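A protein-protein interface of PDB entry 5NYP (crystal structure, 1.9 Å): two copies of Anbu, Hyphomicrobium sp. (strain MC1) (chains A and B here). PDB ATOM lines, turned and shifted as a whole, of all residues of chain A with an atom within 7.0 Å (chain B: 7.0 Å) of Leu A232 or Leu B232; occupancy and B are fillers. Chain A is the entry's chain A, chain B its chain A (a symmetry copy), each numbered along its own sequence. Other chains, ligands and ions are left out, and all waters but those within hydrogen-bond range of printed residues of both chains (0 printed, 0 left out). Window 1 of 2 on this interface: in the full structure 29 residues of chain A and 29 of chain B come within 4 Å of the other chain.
The guanidinium group of Arg A163 lies within hydrogen-bond range of the backbone carbonyl oxygen of Ser B225 (3.0 Å).
The guanidinium group (NH1) of Arg A163 lies within hydrogen-bond range of the side-chain hydroxyl (OG) of Ser B229 (2.6 Å).
NE of Arg B233 is in hydrogen-bond range of O of Arg A163.
The guanidinium group (NH1) of Arg B163 lies within hydrogen-bond range of the backbone carbonyl oxygen (O) of Ser A225, 3.0 Å away.
The guanidinium group of Arg B163 lies within hydrogen-bond range of the side-chain hydroxyl of Ser A229, at 2.6 Å.
NE of Arg A233 lies within hydrogen-bond range of O of Arg B163, at 3.1 Å.
OG of Ser A229 lies within hydrogen-bond range of O of Ser A225, at 3.3 Å.
OD1 of Asp A230 lies within salt-bridge range of NH1 of Arg A233 (2.7 Å).
O of Arg A233 sits at hydrogen-bond distance from OG of Ser A237 (3.0 Å).
The backbone carbonyl oxygen of Ser B225 is in hydrogen-bond range of the side-chain hydroxyl of Ser B229 (3.3 Å).
NH1 of Arg B233 lies within salt-bridge range of OD1 of Asp B230 (2.7 Å).
The side-chain hydroxyl of Ser B237 sits at hydrogen-bond distance from the backbone carbonyl oxygen of Arg B233 (3.0 Å).
Among the printed residues, pairs that only touch across the chains: Ile A160 with Ile B160 (3.6 Å), Ile A160 with Leu B232 (3.6 Å), Arg A163 with Trp B228 (3.8 Å), Arg A163 with Leu B232 (3.5 Å), Val A164 with Leu B232 (3.8 Å), Val A164 with Phe B236 (3.9 Å), Ala A227 with Ile B239 (3.4 Å), Trp A228 with Arg B163 (3.8 Å), Trp A228 with Ala B235 (3.9 Å), Trp A228 with Phe B236 (3.6 Å), Trp A228 with Ile B239 (3.3 Å), Ala A231 with Ala B235 (3.9 Å), Ala A231 with Ile B239 (3.7 Å), Leu A232 with Ile B160 (3.6 Å), Leu A232 with Arg B163 (3.5 Å), Leu A232 with Val B164 (3.8 Å), Leu A232 with Leu B232 (3.3 Å), Ala A235 with Trp B228 (3.9 Å), Ala A235 with Ala B231 (3.9 Å), Phe A236 with Val B164 (3.9 Å), Phe A236 with Trp B228 (3.6 Å), Ile A239 with Ala B227 (3.4 Å), Ile A239 with Trp B228 (3.3 Å) and Ile A239 with Ala B231 (3.7 Å).
Of the printed residues of chain B, Ala A227 touches Ile B239 (3.4 Å).
Of the printed residues of chain B, Ala A235 touches Trp B228 (3.9 Å) and Ala B231 (3.9 Å).
Pro B159 touches none of the printed residues of chain A.
Of the printed residues of chain A, Val B164 touches Leu A232 and Phe A236.
Of chain A, only Ile A160 (3.6 Å), Arg A163 (3.5 Å), Val A164 (3.8 Å) and Leu A232 (3.3 Å) come within 4 Å of Leu B232.
Lys B238 touches none of the printed residues of chain A.
The nearest printed residue of chain A that does not touch Ser B225 is Ile A239 (6.5 Å).
Of the 18 printed residues of chain B, 13 touch a printed residue of chain A.
Hydrophobic or aromatic side chains of chain B within 4 Å of the printed part of chain A: Ile B160, Val B164, Ala B227, Trp B228, Ala B231, Leu B232, Ala B235, Phe B236 and Ile B239.
Of the 18 printed residues of chain A, 13 touch a printed residue of chain B.
Hydrophobic or aromatic side chains of chain A within 4 Å of the printed part of chain B: Ile A160, Val A164, Ala A227, Trp A228, Ala A231, Leu A232, Ala A235, Phe A236 and Ile A239.
Among the printed residues, 30 pairs touch across the chains.
Among the printed residues, no Asp or Glu carboxylate lies within 4 Å of a Lys or Arg side-chain nitrogen of the other chain.
Ile A160 touches Leu B232, and with the chains exchanged Leu A232 touches Ile B160.
Arg A163 touches Leu B232, and with the chains exchanged Leu A232 touches Arg B163.
Val A164 touches Phe B236, and with the chains exchanged Phe A236 touches Val B164.
Trp A228 touches Phe B236, and with the chains exchanged Phe A236 touches Trp B228.
Positions printed for both chains: 159, 160, 163, 164, 225, 227, 228, 229, 230, 231, 232, 233, 234, 235, 236, 237, 238 and 239.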
ATOM      1  N   PRO A 159      -8.635 -16.711  26.167  1.00  0.00           N
ATOM      2  CA  PRO A 159     -10.021 -17.010  26.561  1.00  0.00           C
ATOM      3  C   PRO A 159     -10.164 -18.227  27.479  1.00  0.00           C
ATOM      4  O   PRO A 159     -10.981 -18.200  28.397  1.00  0.00           O
ATOM      5  CB  PRO A 159     -10.723 -17.266  25.217  1.00  0.00           C
ATOM      6  CG  PRO A 159      -9.912 -16.520  24.221  1.00  0.00           C
ATOM      7  CD  PRO A 159      -8.498 -16.673  24.697  1.00  0.00           C
ATOM      8  N   ILE A 160      -9.361 -19.263  27.242  1.00  0.00           N
ATOM      9  CA  ILE A 160      -9.387 -20.476  28.061  1.00  0.00           C
ATOM     10  C   ILE A 160      -8.840 -20.207  29.464  1.00  0.00           C
ATOM     11  O   ILE A 160      -9.424 -20.659  30.451  1.00  0.00           O
ATOM     12  CB  ILE A 160      -8.604 -21.635  27.394  1.00  0.00           C
ATOM     13  CG1 ILE A 160      -9.184 -21.967  26.003  1.00  0.00           C
ATOM     14  CG2 ILE A 160      -8.601 -22.881  28.275  1.00  0.00           C
ATOM     15  CD1 ILE A 160     -10.683 -22.206  25.962  1.00  0.00           C
ATOM     16  N   ARG A 163     -11.406 -18.212  31.520  1.00  0.00           N
ATOM     17  CA  ARG A 163     -12.562 -19.010  31.953  1.00  0.00           C
ATOM     18  C   ARG A 163     -12.225 -20.114  32.966  1.00  0.00           C
ATOM     19  O   ARG A 163     -13.074 -20.470  33.789  1.00  0.00           O
ATOM     20  CB  ARG A 163     -13.244 -19.645  30.734  1.00  0.00           C
ATOM     21  CG  ARG A 163     -13.853 -18.649  29.750  1.00  0.00           C
ATOM     22  CD  ARG A 163     -14.111 -19.308  28.403  1.00  0.00           C
ATOM     23  NE  ARG A 163     -14.645 -18.388  27.396  1.00  0.00           N
ATOM     24  CZ  ARG A 163     -15.935 -18.085  27.215  1.00  0.00           C
ATOM     25  NH1 ARG A 163     -16.896 -18.610  27.977  1.00  0.00           N
ATOM     26  NH2 ARG A 163     -16.273 -17.235  26.248  1.00  0.00           N
ATOM     27  N   VAL A 164     -11.005 -20.655  32.898  1.00  0.00           N
ATOM     28  CA  VAL A 164     -10.620 -21.846  33.678  1.00  0.00           C
ATOM     29  C   VAL A 164      -9.680 -21.553  34.864  1.00  0.00           C
ATOM     30  O   VAL A 164      -9.798 -22.199  35.905  1.00  0.00           O
ATOM     31  CB  VAL A 164     -10.010 -22.929  32.751  1.00  0.00           C
ATOM     32  CG1 VAL A 164      -9.600 -24.174  33.532  1.00  0.00           C
ATOM     33  CG2 VAL A 164     -11.010 -23.309  31.663  1.00  0.00           C
ATOM     34  N   SER A 225      -2.171 -33.022  25.662  1.00  0.00           N
ATOM     35  CA  SER A 225      -2.772 -32.240  24.577  1.00  0.00           C
ATOM     36  C   SER A 225      -3.848 -33.020  23.814  1.00  0.00           C
ATOM     37  O   SER A 225      -4.901 -32.467  23.495  1.00  0.00           O
ATOM     38  CB  SER A 225      -1.694 -31.745  23.606  1.00  0.00           C
ATOM     39  OG  SER A 225      -2.261 -30.938  22.587  1.00  0.00           O
ATOM     40  N   ALA A 227      -5.688 -35.520  25.015  1.00  0.00           N
ATOM     41  CA  ALA A 227      -6.832 -35.619  25.927  1.00  0.00           C
ATOM     42  C   ALA A 227      -7.609 -34.302  26.026  1.00  0.00           C
ATOM     43  O   ALA A 227      -8.834 -34.317  26.120  1.00  0.00           O
ATOM     44  CB  ALA A 227      -6.380 -36.075  27.311  1.00  0.00           C
ATOM     45  N   TRP A 228      -6.895 -33.174  26.003  1.00  0.00           N
ATOM     46  CA  TRP A 228      -7.526 -31.846  26.001  1.00  0.00           C
ATOM     47  C   TRP A 228      -8.421 -31.652  24.770  1.00  0.00           C
ATOM     48  O   TRP A 228      -9.571 -31.229  24.901  1.00  0.00           O
ATOM     49  CB  TRP A 228      -6.458 -30.752  26.086  1.00  0.00           C
ATOM     50  CG  TRP A 228      -6.965 -29.327  26.140  1.00  0.00           C
ATOM     51  CD1 TRP A 228      -6.556 -28.292  25.349  1.00  0.00           C
ATOM     52  CD2 TRP A 228      -7.945 -28.781  27.038  1.00  0.00           C
ATOM     53  NE1 TRP A 228      -7.220 -27.141  25.691  1.00  0.00           N
ATOM     54  CE2 TRP A 228      -8.079 -27.410  26.723  1.00  0.00           C
ATOM     55  CE3 TRP A 228      -8.727 -29.314  28.074  1.00  0.00           C
ATOM     56  CZ2 TRP A 228      -8.960 -26.563  27.407  1.00  0.00           C
ATOM     57  CZ3 TRP A 228      -9.607 -28.471  28.755  1.00  0.00           C
ATOM     58  CH2 TRP A 228      -9.714 -27.110  28.414  1.00  0.00           C
ATOM     59  N   SER A 229      -7.898 -31.988  23.591  1.00  0.00           N
ATOM     60  CA  SER A 229      -8.680 -31.944  22.344  1.00  0.00           C
ATOM     61  C   SER A 229      -9.948 -32.791  22.428  1.00  0.00           C
ATOM     62  O   SER A 229     -11.028 -32.328  22.056  1.00  0.00           O
ATOM     63  CB  SER A 229      -7.842 -32.412  21.154  1.00  0.00           C
ATOM     64  OG  SER A 229      -6.742 -31.553  20.946  1.00  0.00           O
ATOM     65  N   ASP A 230      -9.804 -34.023  22.924  1.00  0.00           N
ATOM     66  CA  ASP A 230     -10.942 -34.926  23.146  1.00  0.00           C
ATOM     67  C   ASP A 230     -11.964 -34.318  24.105  1.00  0.00           C
ATOM     68  O   ASP A 230     -13.165 -34.369  23.846  1.00  0.00           O
ATOM     69  CB  ASP A 230     -10.475 -36.283  23.705  1.00  0.00           C
ATOM     70  CG  ASP A 230      -9.691 -37.116  22.692  1.00  0.00           C
ATOM     71  OD1 ASP A 230      -9.479 -36.667  21.546  1.00  0.00           O
ATOM     72  OD2 ASP A 230      -9.279 -38.240  23.055  1.00  0.00           O
ATOM     73  N   ALA A 231     -11.475 -33.750  25.207  1.00  0.00           N
ATOM     74  CA  ALA A 231     -12.331 -33.116  26.211  1.00  0.00           C
ATOM     75  C   ALA A 231     -13.040 -31.868  25.674  1.00  0.00           C
ATOM     76  O   ALA A 231     -14.198 -31.623  26.016  1.00  0.00           O
ATOM     77  CB  ALA A 231     -11.520 -32.767  27.452  1.00  0.00           C
ATOM     78  N   LEU A 232     -12.345 -31.088  24.847  1.00  0.00           N
ATOM     79  CA  LEU A 232     -12.945 -29.910  24.204  1.00  0.00           C
ATOM     80  C   LEU A 232     -14.084 -30.278  23.255  1.00  0.00           C
ATOM     81  O   LEU A 232     -15.130 -29.623  23.261  1.00  0.00           O
ATOM     82  CB  LEU A 232     -11.888 -29.091  23.455  1.00  0.00           C
ATOM     83  CG  LEU A 232     -10.941 -28.260  24.326  1.00  0.00           C
ATOM     84  CD1 LEU A 232      -9.779 -27.759  23.487  1.00  0.00           C
ATOM     85  CD2 LEU A 232     -11.672 -27.098  24.986  1.00  0.00           C
ATOM     86  N   ARG A 233     -13.879 -31.319  22.448  1.00  0.00           N
ATOM     87  CA  ARG A 233     -14.920 -31.805  21.534  1.00  0.00           C
ATOM     88  C   ARG A 233     -16.145 -32.297  22.299  1.00  0.00           C
ATOM     89  O   ARG A 233     -17.276 -31.999  21.917  1.00  0.00           O
ATOM     90  CB  ARG A 233     -14.385 -32.917  20.629  1.00  0.00           C
ATOM     91  CG  ARG A 233     -13.349 -32.441  19.624  1.00  0.00           C
ATOM     92  CD  ARG A 233     -12.935 -33.542  18.660  1.00  0.00           C
ATOM     93  NE  ARG A 233     -11.498 -33.485  18.367  1.00  0.00           N
ATOM     94  CZ  ARG A 233     -10.557 -34.307  18.850  1.00  0.00           C
ATOM     95  NH1 ARG A 233     -10.846 -35.310  19.680  1.00  0.00           N
ATOM     96  NH2 ARG A 233      -9.289 -34.124  18.486  1.00  0.00           N
ATOM     97  N   GLN A 234     -15.909 -33.038  23.380  1.00  0.00           N
ATOM     98  CA  GLN A 234     -16.982 -33.461  24.282  1.00  0.00           C
ATOM     99  C   GLN A 234     -17.667 -32.260  24.941  1.00  0.00           C
ATOM    100  O   GLN A 234     -18.891 -32.227  25.032  1.00  0.00           O
ATOM    101  CB  GLN A 234     -16.452 -34.428  25.348  1.00  0.00           C
ATOM    102  CG  GLN A 234     -16.047 -35.783  24.789  1.00  0.00           C
ATOM    103  CD  GLN A 234     -15.439 -36.698  25.839  1.00  0.00           C
ATOM    104  OE1 GLN A 234     -16.112 -37.096  26.791  1.00  0.00           O
ATOM    105  NE2 GLN A 234     -14.168 -37.045  25.664  1.00  0.00           N
ATOM    106  N   ALA A 235     -16.879 -31.279  25.377  1.00  0.00           N
ATOM    107  CA  ALA A 235     -17.413 -30.045  25.968  1.00  0.00           C
ATOM    108  C   ALA A 235     -18.318 -29.286  24.992  1.00  0.00           C
ATOM    109  O   ALA A 235     -19.406 -28.832  25.368  1.00  0.00           O
ATOM    110  CB  ALA A 235     -16.281 -29.146  26.447  1.00  0.00           C
ATOM    111  N   PHE A 236     -17.881 -29.166  23.741  1.00  0.00           N
ATOM    112  CA  PHE A 236     -18.697 -28.513  22.721  1.00  0.00           C
ATOM    113  C   PHE A 236     -19.968 -29.307  22.399  1.00  0.00           C
ATOM    114  O   PHE A 236     -21.034 -28.716  22.216  1.00  0.00           O
ATOM    115  CB  PHE A 236     -17.908 -28.242  21.440  1.00  0.00           C
ATOM    116  CG  PHE A 236     -18.675 -27.423  20.445  1.00  0.00           C
ATOM    117  CD1 PHE A 236     -18.890 -26.069  20.670  1.00  0.00           C
ATOM    118  CD2 PHE A 236     -19.236 -28.013  19.317  1.00  0.00           C
ATOM    119  CE1 PHE A 236     -19.623 -25.309  19.774  1.00  0.00           C
ATOM    120  CE2 PHE A 236     -19.969 -27.258  18.416  1.00  0.00           C
ATOM    121  CZ  PHE A 236     -20.161 -25.905  18.645  1.00  0.00           C
ATOM    122  N   SER A 237     -19.852 -30.635  22.339  1.00  0.00           N
ATOM    123  CA  SER A 237     -21.009 -31.513  22.123  1.00  0.00           C
ATOM    124  C   SER A 237     -22.103 -31.354  23.184  1.00  0.00           C
ATOM    125  O   SER A 237     -23.279 -31.525  22.877  1.00  0.00           O
ATOM    126  CB  SER A 237     -20.580 -32.983  22.043  1.00  0.00           C
ATOM    127  OG  SER A 237     -19.818 -33.221  20.874  1.00  0.00           O
ATOM    128  N   LYS A 238     -21.715 -31.035  24.418  1.00  0.00           N
ATOM    129  CA  LYS A 238     -22.680 -30.752  25.487  1.00  0.00           C
ATOM    130  C   LYS A 238     -23.379 -29.413  25.233  1.00  0.00           C
ATOM    131  O   LYS A 238     -24.609 -29.355  25.159  1.00  0.00           O
ATOM    132  CB  LYS A 238     -21.996 -30.713  26.859  1.00  0.00           C
ATOM    133  CG  LYS A 238     -21.344 -32.017  27.298  1.00  0.00           C
ATOM    134  CD  LYS A 238     -22.353 -33.042  27.789  1.00  0.00           C
ATOM    135  CE  LYS A 238     -21.642 -34.273  28.331  1.00  0.00           C
ATOM    136  NZ  LYS A 238     -22.592 -35.295  28.852  1.00  0.00           N
ATOM    137  N   ILE A 239     -22.586 -28.353  25.079  1.00  0.00           N
ATOM    138  CA  ILE A 239     -23.119 -26.981  25.010  1.00  0.00           C
ATOM    139  C   ILE A 239     -23.844 -26.616  23.710  1.00  0.00           C
ATOM    140  O   ILE A 239     -24.542 -25.603  23.670  1.00  0.00           O
ATOM    141  CB  ILE A 239     -22.042 -25.901  25.300  1.00  0.00           C
ATOM    142  CG1 ILE A 239     -20.939 -25.890  24.229  1.00  0.00           C
ATOM    143  CG2 ILE A 239     -21.460 -26.096  26.696  1.00  0.00           C
ATOM    144  CD1 ILE A 239     -20.483 -24.499  23.847  1.00  0.00           C
ATOM    145  N   PRO B 159      -6.677 -21.993  18.799  1.00  0.00           N
ATOM    146  CA  PRO B 159      -6.460 -23.362  19.291  1.00  0.00           C
ATOM    147  C   PRO B 159      -7.742 -24.182  19.454  1.00  0.00           C
ATOM    148  O   PRO B 159      -7.739 -25.374  19.155  1.00  0.00           O
ATOM    149  CB  PRO B 159      -5.784 -23.144  20.655  1.00  0.00           C
ATOM    150  CG  PRO B 159      -5.139 -21.809  20.547  1.00  0.00           C
ATOM    151  CD  PRO B 159      -6.093 -20.998  19.721  1.00  0.00           C
ATOM    152  N   ILE B 160      -8.819 -23.540  19.901  1.00  0.00           N
ATOM    153  CA  ILE B 160     -10.109 -24.208  20.080  1.00  0.00           C
ATOM    154  C   ILE B 160     -10.730 -24.582  18.733  1.00  0.00           C
ATOM    155  O   ILE B 160     -11.240 -25.693  18.576  1.00  0.00           O
ATOM    156  CB  ILE B 160     -11.095 -23.339  20.902  1.00  0.00           C
ATOM    157  CG1 ILE B 160     -10.515 -23.006  22.292  1.00  0.00           C
ATOM    158  CG2 ILE B 160     -12.450 -24.026  21.046  1.00  0.00           C
ATOM    159  CD1 ILE B 160     -10.016 -24.196  23.092  1.00  0.00           C
ATOM    160  N   ARG B 163      -8.869 -27.584  17.211  1.00  0.00           N
ATOM    161  CA  ARG B 163      -9.163 -28.859  17.880  1.00  0.00           C
ATOM    162  C   ARG B 163     -10.611 -29.343  17.709  1.00  0.00           C
ATOM    163  O   ARG B 163     -10.857 -30.553  17.718  1.00  0.00           O
ATOM    164  CB  ARG B 163      -8.848 -28.750  19.377  1.00  0.00           C
ATOM    165  CG  ARG B 163      -7.377 -28.512  19.706  1.00  0.00           C
ATOM    166  CD  ARG B 163      -7.218 -27.993  21.127  1.00  0.00           C
ATOM    167  NE  ARG B 163      -5.829 -27.692  21.487  1.00  0.00           N
ATOM    168  CZ  ARG B 163      -4.937 -28.563  21.970  1.00  0.00           C
ATOM    169  NH1 ARG B 163      -5.241 -29.849  22.168  1.00  0.00           N
ATOM    170  NH2 ARG B 163      -3.709 -28.142  22.261  1.00  0.00           N
ATOM    171  N   VAL B 164     -11.555 -28.408  17.569  1.00  0.00           N
ATOM    172  CA  VAL B 164     -12.996 -28.726  17.588  1.00  0.00           C
ATOM    173  C   VAL B 164     -13.682 -28.657  16.210  1.00  0.00           C
ATOM    174  O   VAL B 164     -14.576 -29.457  15.938  1.00  0.00           O
ATOM    175  CB  VAL B 164     -13.735 -27.827  18.615  1.00  0.00           C
ATOM    176  CG1 VAL B 164     -15.230 -28.133  18.656  1.00  0.00           C
ATOM    177  CG2 VAL B 164     -13.132 -28.014  20.004  1.00  0.00           C
ATOM    178  N   SER B 225     -22.243 -18.689  26.210  1.00  0.00           N
ATOM    179  CA  SER B 225     -20.901 -18.412  26.733  1.00  0.00           C
ATOM    180  C   SER B 225     -20.716 -18.906  28.171  1.00  0.00           C
ATOM    181  O   SER B 225     -19.674 -19.476  28.499  1.00  0.00           O
ATOM    182  CB  SER B 225     -20.584 -16.916  26.646  1.00  0.00           C
ATOM    183  OG  SER B 225     -19.266 -16.648  27.096  1.00  0.00           O
ATOM    184  N   ALA B 227     -22.372 -21.402  29.624  1.00  0.00           N
ATOM    185  CA  ALA B 227     -22.320 -22.865  29.541  1.00  0.00           C
ATOM    186  C   ALA B 227     -20.973 -23.368  29.009  1.00  0.00           C
ATOM    187  O   ALA B 227     -20.477 -24.395  29.468  1.00  0.00           O
ATOM    188  CB  ALA B 227     -23.463 -23.397  28.681  1.00  0.00           C
ATOM    189  N   TRP B 228     -20.392 -22.644  28.050  1.00  0.00           N
ATOM    190  CA  TRP B 228     -19.060 -22.971  27.520  1.00  0.00           C
ATOM    191  C   TRP B 228     -17.990 -22.914  28.618  1.00  0.00           C
ATOM    192  O   TRP B 228     -17.197 -23.847  28.758  1.00  0.00           O
ATOM    193  CB  TRP B 228     -18.709 -22.036  26.358  1.00  0.00           C
ATOM    194  CG  TRP B 228     -17.380 -22.286  25.680  1.00  0.00           C
ATOM    195  CD1 TRP B 228     -16.412 -21.355  25.428  1.00  0.00           C
ATOM    196  CD2 TRP B 228     -16.886 -23.528  25.151  1.00  0.00           C
ATOM    197  NE1 TRP B 228     -15.350 -21.936  24.783  1.00  0.00           N
ATOM    198  CE2 TRP B 228     -15.611 -23.268  24.601  1.00  0.00           C
ATOM    199  CE3 TRP B 228     -17.393 -24.835  25.092  1.00  0.00           C
ATOM    200  CZ2 TRP B 228     -14.834 -24.264  23.996  1.00  0.00           C
ATOM    201  CZ3 TRP B 228     -16.618 -25.829  24.492  1.00  0.00           C
ATOM    202  CH2 TRP B 228     -15.352 -25.534  23.953  1.00  0.00           C
ATOM    203  N   SER B 229     -17.996 -21.838  29.404  1.00  0.00           N
ATOM    204  CA  SER B 229     -17.087 -21.703  30.555  1.00  0.00           C
ATOM    205  C   SER B 229     -17.225 -22.864  31.538  1.00  0.00           C
ATOM    206  O   SER B 229     -16.220 -23.434  31.967  1.00  0.00           O
ATOM    207  CB  SER B 229     -17.333 -20.388  31.295  1.00  0.00           C
ATOM    208  OG  SER B 229     -17.059 -19.283  30.462  1.00  0.00           O
ATOM    209  N   ASP B 230     -18.470 -23.207  31.878  1.00  0.00           N
ATOM    210  CA  ASP B 230     -18.768 -24.355  32.745  1.00  0.00           C
ATOM    211  C   ASP B 230     -18.232 -25.660  32.156  1.00  0.00           C
ATOM    212  O   ASP B 230     -17.626 -26.459  32.866  1.00  0.00           O
ATOM    213  CB  ASP B 230     -20.283 -24.497  32.982  1.00  0.00           C
ATOM    214  CG  ASP B 230     -20.867 -23.378  33.842  1.00  0.00           C
ATOM    215  OD1 ASP B 230     -20.127 -22.465  34.266  1.00  0.00           O
ATOM    216  OD2 ASP B 230     -22.091 -23.415  34.097  1.00  0.00           O
ATOM    217  N   ALA B 231     -18.465 -25.860  30.858  1.00  0.00           N
ATOM    218  CA  ALA B 231     -18.001 -27.056  30.153  1.00  0.00           C
ATOM    219  C   ALA B 231     -16.474 -27.134  30.068  1.00  0.00           C
ATOM    220  O   ALA B 231     -15.905 -28.221  30.174  1.00  0.00           O
ATOM    221  CB  ALA B 231     -18.609 -27.114  28.758  1.00  0.00           C
ATOM    222  N   LEU B 232     -15.821 -25.988  29.873  1.00  0.00           N
ATOM    223  CA  LEU B 232     -14.353 -25.925  29.857  1.00  0.00           C
ATOM    224  C   LEU B 232     -13.735 -26.302  31.202  1.00  0.00           C
ATOM    225  O   LEU B 232     -12.753 -27.048  31.245  1.00  0.00           O
ATOM    226  CB  LEU B 232     -13.864 -24.535  29.434  1.00  0.00           C
ATOM    227  CG  LEU B 232     -13.996 -24.201  27.945  1.00  0.00           C
ATOM    228  CD1 LEU B 232     -13.770 -22.716  27.728  1.00  0.00           C
ATOM    229  CD2 LEU B 232     -13.028 -25.023  27.104  1.00  0.00           C
ATOM    230  N   ARG B 233     -14.311 -25.791  32.290  1.00  0.00           N
ATOM    231  CA  ARG B 233     -13.847 -26.129  33.641  1.00  0.00           C
ATOM    232  C   ARG B 233     -14.007 -27.618  33.929  1.00  0.00           C
ATOM    233  O   ARG B 233     -13.106 -28.244  34.485  1.00  0.00           O
ATOM    234  CB  ARG B 233     -14.585 -25.307  34.701  1.00  0.00           C
ATOM    235  CG  ARG B 233     -14.251 -23.825  34.666  1.00  0.00           C
ATOM    236  CD  ARG B 233     -14.901 -23.062  35.809  1.00  0.00           C
ATOM    237  NE  ARG B 233     -15.377 -21.745  35.373  1.00  0.00           N
ATOM    238  CZ  ARG B 233     -16.649 -21.396  35.142  1.00  0.00           C
ATOM    239  NH1 ARG B 233     -17.660 -22.251  35.297  1.00  0.00           N
ATOM    240  NH2 ARG B 233     -16.919 -20.153  34.748  1.00  0.00           N
ATOM    241  N   GLN B 234     -15.153 -28.175  33.536  1.00  0.00           N
ATOM    242  CA  GLN B 234     -15.384 -29.618  33.626  1.00  0.00           C
ATOM    243  C   GLN B 234     -14.406 -30.400  32.744  1.00  0.00           C
ATOM    244  O   GLN B 234     -13.870 -31.417  33.175  1.00  0.00           O
ATOM    245  CB  GLN B 234     -16.832 -29.964  33.255  1.00  0.00           C
ATOM    246  CG  GLN B 234     -17.850 -29.483  34.280  1.00  0.00           C
ATOM    247  CD  GLN B 234     -19.285 -29.752  33.857  1.00  0.00           C
ATOM    248  OE1 GLN B 234     -19.697 -30.903  33.729  1.00  0.00           O
ATOM    249  NE2 GLN B 234     -20.054 -28.686  33.651  1.00  0.00           N
ATOM    250  N   ALA B 235     -14.166 -29.911  31.528  1.00  0.00           N
ATOM    251  CA  ALA B 235     -13.200 -30.528  30.609  1.00  0.00           C
ATOM    252  C   ALA B 235     -11.786 -30.560  31.199  1.00  0.00           C
ATOM    253  O   ALA B 235     -11.099 -31.586  31.126  1.00  0.00           O
ATOM    254  CB  ALA B 235     -13.197 -29.806  29.268  1.00  0.00           C
ATOM    255  N   PHE B 236     -11.363 -29.450  31.796  1.00  0.00           N
ATOM    256  CA  PHE B 236     -10.054 -29.399  32.442  1.00  0.00           C
ATOM    257  C   PHE B 236      -9.978 -30.312  33.671  1.00  0.00           C
ATOM    258  O   PHE B 236      -8.957 -30.968  33.888  1.00  0.00           O
ATOM    259  CB  PHE B 236      -9.656 -27.973  32.822  1.00  0.00           C
ATOM    260  CG  PHE B 236      -8.248 -27.877  33.332  1.00  0.00           C
ATOM    261  CD1 PHE B 236      -7.177 -28.006  32.457  1.00  0.00           C
ATOM    262  CD2 PHE B 236      -7.990 -27.720  34.690  1.00  0.00           C
ATOM    263  CE1 PHE B 236      -5.873 -27.950  32.920  1.00  0.00           C
ATOM    264  CE2 PHE B 236      -6.688 -27.661  35.160  1.00  0.00           C
ATOM    265  CZ  PHE B 236      -5.629 -27.775  34.272  1.00  0.00           C
ATOM    266  N   SER B 237     -11.053 -30.356  34.459  1.00  0.00           N
ATOM    267  CA  SER B 237     -11.138 -31.254  35.619  1.00  0.00           C
ATOM    268  C   SER B 237     -10.969 -32.733  35.258  1.00  0.00           C
ATOM    269  O   SER B 237     -10.449 -33.500  36.064  1.00  0.00           O
ATOM    270  CB  SER B 237     -12.458 -31.057  36.374  1.00  0.00           C
ATOM    271  OG  SER B 237     -12.498 -29.785  36.994  1.00  0.00           O
ATOM    272  N   LYS B 238     -11.408 -33.125  34.063  1.00  0.00           N
ATOM    273  CA  LYS B 238     -11.200 -34.492  33.569  1.00  0.00           C
ATOM    274  C   LYS B 238      -9.724 -34.719  33.233  1.00  0.00           C
ATOM    275  O   LYS B 238      -9.097 -35.639  33.765  1.00  0.00           O
ATOM    276  CB  LYS B 238     -12.052 -34.769  32.324  1.00  0.00           C
ATOM    277  CG  LYS B 238     -13.558 -34.686  32.533  1.00  0.00           C
ATOM    278  CD  LYS B 238     -14.121 -35.909  33.235  1.00  0.00           C
ATOM    279  CE  LYS B 238     -15.639 -35.832  33.306  1.00  0.00           C
ATOM    280  NZ  LYS B 238     -16.241 -37.026  33.962  1.00  0.00           N
ATOM    281  N   ILE B 239      -9.177 -33.863  32.370  1.00  0.00           N
ATOM    282  CA  ILE B 239      -7.826 -34.067  31.818  1.00  0.00           C
ATOM    283  C   ILE B 239      -6.668 -33.813  32.790  1.00  0.00           C
ATOM    284  O   ILE B 239      -5.538 -34.209  32.502  1.00  0.00           O
ATOM    285  CB  ILE B 239      -7.576 -33.249  30.521  1.00  0.00           C
ATOM    286  CG1 ILE B 239      -7.611 -31.734  30.782  1.00  0.00           C
ATOM    287  CG2 ILE B 239      -8.576 -33.652  29.442  1.00  0.00           C
ATOM    288  CD1 ILE B 239      -6.557 -30.966  30.017  1.00  0.00           C
